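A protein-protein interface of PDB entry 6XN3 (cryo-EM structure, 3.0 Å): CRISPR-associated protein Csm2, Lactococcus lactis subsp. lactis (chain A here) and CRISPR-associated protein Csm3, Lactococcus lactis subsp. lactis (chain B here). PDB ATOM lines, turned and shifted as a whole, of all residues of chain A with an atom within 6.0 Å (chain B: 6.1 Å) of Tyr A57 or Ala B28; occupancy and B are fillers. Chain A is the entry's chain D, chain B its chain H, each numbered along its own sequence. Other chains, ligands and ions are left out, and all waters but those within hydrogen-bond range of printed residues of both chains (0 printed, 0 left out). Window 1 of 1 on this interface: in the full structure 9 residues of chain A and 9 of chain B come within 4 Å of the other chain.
The side-chain amide nitrogen (ND2) of Asn A58 is in hydrogen-bond range of the backbone carbonyl oxygen (O) of Asn A54, at 2.8 Å.
The backbone carbonyl oxygen (O) of Gly B27 is in hydrogen-bond range of the side-chain amide nitrogen (NE2) of Gln B134 (3.3 Å).
Along chain A the printed residues that touch a printed residue of chain B span positions 54 to 126.
Hydrophobic or aromatic side chains of chain B within 4 Å of the printed part of chain A: Ala B25, Ile B26, Ala B28 and Val B29.
Among the printed residues, no Asp or Glu carboxylate lies within 4 Å of a Lys or Arg side-chain nitrogen of the other chain.
Of chain B, only Ala B25 and Ala B28 come within 4 Å of Tyr A57.
Val A60 touches none of the printed residues of chain B.
Of the printed residues of chain B, Glu A126 touches Ala B25 and Ile B26.
Of the printed residues of chain A, Gly B27 touches Asn A54 (3.3 Å).
The nearest residue of chain B that does not touch Tyr A57 is Phe B23 (4.5 Å).
The nearest printed residue of chain B that does not touch Glu A126 is Ser B24 (5.0 Å).
Gly B27 touches Asn A54 (CA to OD1, 3.3 Å).
Tyr A57 touches Ala B25 (CE2 to CB, 3.6 Å).
Ala B28 touches Tyr A57.
ND2 of Asn A58 touches CB of Ala B28, 3.9 Å away.
Val B29 touches Asn A58.
Glu A126 touches Ala B25 (OE2 to CB, 3.3 Å).
Ile B26 touches Glu A126.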
ATOM      1  N   VAL A  53     -11.431 -30.577   9.520  1.00  0.00           N
ATOM      2  CA  VAL A  53     -10.183 -30.341  10.245  1.00  0.00           C
ATOM      3  C   VAL A  53      -9.197 -29.556   9.389  1.00  0.00           C
ATOM      4  O   VAL A  53      -8.516 -28.649   9.881  1.00  0.00           O
ATOM      5  CB  VAL A  53      -9.576 -31.664  10.739  1.00  0.00           C
ATOM      6  CG1 VAL A  53      -8.407 -31.390  11.655  1.00  0.00           C
ATOM      7  CG2 VAL A  53     -10.601 -32.450  11.501  1.00  0.00           C
ATOM      8  N   ASN A  54      -9.115 -29.867   8.091  1.00  0.00           N
ATOM      9  CA  ASN A  54      -8.084 -29.258   7.254  1.00  0.00           C
ATOM     10  C   ASN A  54      -8.394 -27.819   6.881  1.00  0.00           C
ATOM     11  O   ASN A  54      -7.533 -27.133   6.326  1.00  0.00           O
ATOM     12  CB  ASN A  54      -7.861 -30.071   5.992  1.00  0.00           C
ATOM     13  CG  ASN A  54      -7.219 -31.380   6.273  1.00  0.00           C
ATOM     14  OD1 ASN A  54      -7.568 -32.386   5.682  1.00  0.00           O
ATOM     15  ND2 ASN A  54      -6.266 -31.383   7.187  1.00  0.00           N
ATOM     16  N   LYS A  55      -9.600 -27.334   7.164  1.00  0.00           N
ATOM     17  CA  LYS A  55      -9.809 -25.896   7.088  1.00  0.00           C
ATOM     18  C   LYS A  55      -9.066 -25.169   8.197  1.00  0.00           C
ATOM     19  O   LYS A  55      -8.775 -23.978   8.058  1.00  0.00           O
ATOM     20  CB  LYS A  55     -11.299 -25.571   7.138  1.00  0.00           C
ATOM     21  CG  LYS A  55     -12.039 -25.886   5.853  1.00  0.00           C
ATOM     22  CD  LYS A  55     -13.523 -25.630   5.994  1.00  0.00           C
ATOM     23  CE  LYS A  55     -14.240 -25.820   4.676  1.00  0.00           C
ATOM     24  NZ  LYS A  55     -14.188 -27.223   4.206  1.00  0.00           N
ATOM     25  N   VAL A  56      -8.738 -25.861   9.284  1.00  0.00           N
ATOM     26  CA  VAL A  56      -8.004 -25.276  10.393  1.00  0.00           C
ATOM     27  C   VAL A  56      -6.529 -25.612  10.238  1.00  0.00           C
ATOM     28  O   VAL A  56      -5.664 -24.806  10.595  1.00  0.00           O
ATOM     29  CB  VAL A  56      -8.571 -25.770  11.734  1.00  0.00           C
ATOM     30  CG1 VAL A  56      -7.863 -25.142  12.906  1.00  0.00           C
ATOM     31  CG2 VAL A  56     -10.026 -25.444  11.809  1.00  0.00           C
ATOM     32  N   TYR A  57      -6.236 -26.785   9.666  1.00  0.00           N
ATOM     33  CA  TYR A  57      -4.853 -27.251   9.567  1.00  0.00           C
ATOM     34  C   TYR A  57      -4.026 -26.363   8.649  1.00  0.00           C
ATOM     35  O   TYR A  57      -2.833 -26.153   8.886  1.00  0.00           O
ATOM     36  CB  TYR A  57      -4.807 -28.701   9.082  1.00  0.00           C
ATOM     37  CG  TYR A  57      -3.409 -29.192   8.761  1.00  0.00           C
ATOM     38  CD1 TYR A  57      -2.540 -29.581   9.769  1.00  0.00           C
ATOM     39  CD2 TYR A  57      -2.962 -29.273   7.446  1.00  0.00           C
ATOM     40  CE1 TYR A  57      -1.265 -30.025   9.478  1.00  0.00           C
ATOM     41  CE2 TYR A  57      -1.689 -29.704   7.148  1.00  0.00           C
ATOM     42  CZ  TYR A  57      -0.849 -30.085   8.164  1.00  0.00           C
ATOM     43  OH  TYR A  57       0.416 -30.525   7.853  1.00  0.00           O
ATOM     44  N   ASN A  58      -4.645 -25.819   7.602  1.00  0.00           N
ATOM     45  CA  ASN A  58      -3.908 -24.962   6.684  1.00  0.00           C
ATOM     46  C   ASN A  58      -3.527 -23.627   7.304  1.00  0.00           C
ATOM     47  O   ASN A  58      -2.669 -22.929   6.760  1.00  0.00           O
ATOM     48  CB  ASN A  58      -4.711 -24.728   5.411  1.00  0.00           C
ATOM     49  CG  ASN A  58      -4.622 -25.891   4.458  1.00  0.00           C
ATOM     50  OD1 ASN A  58      -3.594 -26.127   3.834  1.00  0.00           O
ATOM     51  ND2 ASN A  58      -5.725 -26.605   4.309  1.00  0.00           N
ATOM     52  N   ARG A  59      -4.136 -23.257   8.422  1.00  0.00           N
ATOM     53  CA  ARG A  59      -3.765 -22.023   9.090  1.00  0.00           C
ATOM     54  C   ARG A  59      -2.955 -22.261  10.352  1.00  0.00           C
ATOM     55  O   ARG A  59      -2.625 -21.299  11.051  1.00  0.00           O
ATOM     56  CB  ARG A  59      -5.017 -21.223   9.433  1.00  0.00           C
ATOM     57  CG  ARG A  59      -5.770 -20.732   8.222  1.00  0.00           C
ATOM     58  CD  ARG A  59      -6.892 -19.848   8.666  1.00  0.00           C
ATOM     59  NE  ARG A  59      -7.809 -20.601   9.505  1.00  0.00           N
ATOM     60  CZ  ARG A  59      -8.816 -20.063  10.173  1.00  0.00           C
ATOM     61  NH1 ARG A  59      -9.586 -20.830  10.919  1.00  0.00           N
ATOM     62  NH2 ARG A  59      -9.050 -18.762  10.095  1.00  0.00           N
ATOM     63  N   VAL A  60      -2.638 -23.512  10.678  1.00  0.00           N
ATOM     64  CA  VAL A  60      -1.861 -23.785  11.883  1.00  0.00           C
ATOM     65  C   VAL A  60      -0.433 -24.170  11.530  1.00  0.00           C
ATOM     66  O   VAL A  60       0.525 -23.672  12.132  1.00  0.00           O
ATOM     67  CB  VAL A  60      -2.553 -24.863  12.730  1.00  0.00           C
ATOM     68  CG1 VAL A  60      -1.676 -25.285  13.878  1.00  0.00           C
ATOM     69  CG2 VAL A  60      -3.821 -24.307  13.272  1.00  0.00           C
ATOM     70  N   ILE A  61      -0.266 -25.025  10.517  1.00  0.00           N
ATOM     71  CA  ILE A  61       1.068 -25.451  10.101  1.00  0.00           C
ATOM     72  C   ILE A  61       1.801 -24.304   9.412  1.00  0.00           C
ATOM     73  O   ILE A  61       3.035 -24.291   9.328  1.00  0.00           O
ATOM     74  CB  ILE A  61       0.949 -26.704   9.206  1.00  0.00           C
ATOM     75  CG1 ILE A  61       2.302 -27.385   8.999  1.00  0.00           C
ATOM     76  CG2 ILE A  61       0.339 -26.357   7.869  1.00  0.00           C
ATOM     77  CD1 ILE A  61       2.883 -27.968  10.257  1.00  0.00           C
ATOM     78  N   ASN A  62       1.062 -23.295   8.978  1.00  0.00           N
ATOM     79  CA  ASN A  62       1.590 -22.112   8.322  1.00  0.00           C
ATOM     80  C   ASN A  62       2.113 -21.092   9.325  1.00  0.00           C
ATOM     81  O   ASN A  62       2.762 -20.112   8.957  1.00  0.00           O
ATOM     82  CB  ASN A  62       0.501 -21.485   7.470  1.00  0.00           C
ATOM     83  CG  ASN A  62       1.013 -20.995   6.175  1.00  0.00           C
ATOM     84  OD1 ASN A  62       1.677 -21.730   5.446  1.00  0.00           O
ATOM     85  ND2 ASN A  62       0.726 -19.738   5.870  1.00  0.00           N
ATOM     86  N   PHE A 118      -3.024 -29.746  18.594  1.00  0.00           N
ATOM     87  CA  PHE A 118      -3.894 -29.780  17.426  1.00  0.00           C
ATOM     88  C   PHE A 118      -3.213 -30.465  16.256  1.00  0.00           C
ATOM     89  O   PHE A 118      -3.872 -31.141  15.461  1.00  0.00           O
ATOM     90  CB  PHE A 118      -4.334 -28.377  17.018  1.00  0.00           C
ATOM     91  CG  PHE A 118      -4.944 -28.328  15.652  1.00  0.00           C
ATOM     92  CD1 PHE A 118      -6.175 -28.899  15.425  1.00  0.00           C
ATOM     93  CD2 PHE A 118      -4.272 -27.754  14.589  1.00  0.00           C
ATOM     94  CE1 PHE A 118      -6.737 -28.884  14.173  1.00  0.00           C
ATOM     95  CE2 PHE A 118      -4.829 -27.744  13.334  1.00  0.00           C
ATOM     96  CZ  PHE A 118      -6.064 -28.303  13.129  1.00  0.00           C
ATOM     97  N   LEU A 119      -1.901 -30.293  16.125  1.00  0.00           N
ATOM     98  CA  LEU A 119      -1.195 -30.957  15.039  1.00  0.00           C
ATOM     99  C   LEU A 119      -1.196 -32.466  15.230  1.00  0.00           C
ATOM    100  O   LEU A 119      -1.368 -33.211  14.262  1.00  0.00           O
ATOM    101  CB  LEU A 119       0.223 -30.418  14.929  1.00  0.00           C
ATOM    102  CG  LEU A 119       0.252 -29.016  14.334  1.00  0.00           C
ATOM    103  CD1 LEU A 119       1.644 -28.449  14.417  1.00  0.00           C
ATOM    104  CD2 LEU A 119      -0.230 -29.053  12.906  1.00  0.00           C
ATOM    105  N   ALA A 122      -4.612 -33.599  14.218  1.00  0.00           N
ATOM    106  CA  ALA A 122      -4.687 -33.679  12.763  1.00  0.00           C
ATOM    107  C   ALA A 122      -3.993 -34.928  12.236  1.00  0.00           C
ATOM    108  O   ALA A 122      -4.483 -35.557  11.287  1.00  0.00           O
ATOM    109  CB  ALA A 122      -4.078 -32.427  12.146  1.00  0.00           C
ATOM    110  N   GLU A 126      -6.059 -37.786  10.140  1.00  0.00           N
ATOM    111  CA  GLU A 126      -5.532 -38.232   8.856  1.00  0.00           C
ATOM    112  C   GLU A 126      -5.181 -39.710   8.887  1.00  0.00           C
ATOM    113  O   GLU A 126      -5.404 -40.426   7.909  1.00  0.00           O
ATOM    114  CB  GLU A 126      -4.314 -37.400   8.473  1.00  0.00           C
ATOM    115  CG  GLU A 126      -4.661 -36.008   8.008  1.00  0.00           C
ATOM    116  CD  GLU A 126      -3.568 -35.008   8.297  1.00  0.00           C
ATOM    117  OE1 GLU A 126      -2.385 -35.399   8.268  1.00  0.00           O
ATOM    118  OE2 GLU A 126      -3.890 -33.828   8.546  1.00  0.00           O
ATOM    119  N   PHE B  23       6.203 -31.805   5.234  1.00  0.00           N
ATOM    120  CA  PHE B  23       5.269 -32.897   5.051  1.00  0.00           C
ATOM    121  C   PHE B  23       3.919 -32.355   4.603  1.00  0.00           C
ATOM    122  O   PHE B  23       3.599 -31.179   4.783  1.00  0.00           O
ATOM    123  CB  PHE B  23       5.120 -33.704   6.333  1.00  0.00           C
ATOM    124  CG  PHE B  23       5.999 -34.910   6.387  1.00  0.00           C
ATOM    125  CD1 PHE B  23       5.590 -36.099   5.817  1.00  0.00           C
ATOM    126  CD2 PHE B  23       7.227 -34.859   7.012  1.00  0.00           C
ATOM    127  CE1 PHE B  23       6.389 -37.210   5.865  1.00  0.00           C
ATOM    128  CE2 PHE B  23       8.032 -35.972   7.063  1.00  0.00           C
ATOM    129  CZ  PHE B  23       7.610 -37.148   6.489  1.00  0.00           C
ATOM    130  N   SER B  24       3.120 -33.228   4.006  1.00  0.00           N
ATOM    131  CA  SER B  24       1.806 -32.859   3.503  1.00  0.00           C
ATOM    132  C   SER B  24       0.746 -33.652   4.244  1.00  0.00           C
ATOM    133  O   SER B  24       0.995 -34.787   4.656  1.00  0.00           O
ATOM    134  CB  SER B  24       1.699 -33.121   2.001  1.00  0.00           C
ATOM    135  OG  SER B  24       2.600 -32.310   1.274  1.00  0.00           O
ATOM    136  N   ALA B  25      -0.427 -33.053   4.424  1.00  0.00           N
ATOM    137  CA  ALA B  25      -1.572 -33.793   4.933  1.00  0.00           C
ATOM    138  C   ALA B  25      -2.270 -34.514   3.790  1.00  0.00           C
ATOM    139  O   ALA B  25      -1.850 -34.396   2.636  1.00  0.00           O
ATOM    140  CB  ALA B  25      -2.543 -32.872   5.659  1.00  0.00           C
ATOM    141  N   ILE B  26      -3.339 -35.250   4.083  1.00  0.00           N
ATOM    142  CA  ILE B  26      -3.975 -36.039   3.037  1.00  0.00           C
ATOM    143  C   ILE B  26      -5.347 -35.465   2.729  1.00  0.00           C
ATOM    144  O   ILE B  26      -6.174 -36.101   2.066  1.00  0.00           O
ATOM    145  CB  ILE B  26      -4.062 -37.521   3.450  1.00  0.00           C
ATOM    146  CG1 ILE B  26      -5.081 -37.727   4.564  1.00  0.00           C
ATOM    147  CG2 ILE B  26      -2.728 -38.022   3.940  1.00  0.00           C
ATOM    148  CD1 ILE B  26      -5.395 -39.164   4.809  1.00  0.00           C
ATOM    149  N   GLY B  27      -5.555 -34.214   3.107  1.00  0.00           N
ATOM    150  CA  GLY B  27      -6.755 -33.500   2.730  1.00  0.00           C
ATOM    151  C   GLY B  27      -6.444 -32.042   2.508  1.00  0.00           C
ATOM    152  O   GLY B  27      -7.342 -31.217   2.343  1.00  0.00           O
ATOM    153  N   ALA B  28      -5.153 -31.725   2.498  1.00  0.00           N
ATOM    154  CA  ALA B  28      -4.673 -30.352   2.488  1.00  0.00           C
ATOM    155  C   ALA B  28      -3.771 -30.120   1.292  1.00  0.00           C
ATOM    156  O   ALA B  28      -3.802 -30.893   0.331  1.00  0.00           O
ATOM    157  CB  ALA B  28      -3.929 -30.017   3.777  1.00  0.00           C
ATOM    158  N   VAL B  29      -3.004 -29.028   1.336  1.00  0.00           N
ATOM    159  CA  VAL B  29      -2.241 -28.572   0.184  1.00  0.00           C
ATOM    160  C   VAL B  29      -1.159 -29.569  -0.195  1.00  0.00           C
ATOM    161  O   VAL B  29      -0.488 -30.158   0.660  1.00  0.00           O
ATOM    162  CB  VAL B  29      -1.652 -27.180   0.458  1.00  0.00           C
ATOM    163  CG1 VAL B  29      -2.751 -26.195   0.585  1.00  0.00           C
ATOM    164  CG2 VAL B  29      -0.852 -27.164   1.752  1.00  0.00           C
ATOM    165  N   ALA B  30      -1.046 -29.817  -1.487  1.00  0.00           N
ATOM    166  CA  ALA B  30       0.127 -30.430  -2.075  1.00  0.00           C
ATOM    167  C   ALA B  30       0.833 -29.346  -2.864  1.00  0.00           C
ATOM    168  O   ALA B  30       0.178 -28.476  -3.447  1.00  0.00           O
ATOM    169  CB  ALA B  30      -0.240 -31.601  -2.971  1.00  0.00           C
ATOM    170  N   GLN B 134      -4.995 -29.113  -4.329  1.00  0.00           N
ATOM    171  CA  GLN B 134      -5.009 -27.850  -3.618  1.00  0.00           C
ATOM    172  C   GLN B 134      -3.600 -27.291  -3.613  1.00  0.00           C
ATOM    173  O   GLN B 134      -2.667 -27.961  -3.164  1.00  0.00           O
ATOM    174  CB  GLN B 134      -5.516 -28.033  -2.191  1.00  0.00           C
ATOM    175  CG  GLN B 134      -6.910 -28.584  -2.114  1.00  0.00           C
ATOM    176  CD  GLN B 134      -7.352 -28.821  -0.702  1.00  0.00           C
ATOM    177  OE1 GLN B 134      -6.884 -28.161   0.221  1.00  0.00           O
ATOM    178  NE2 GLN B 134      -8.261 -29.766  -0.518  1.00  0.00           N
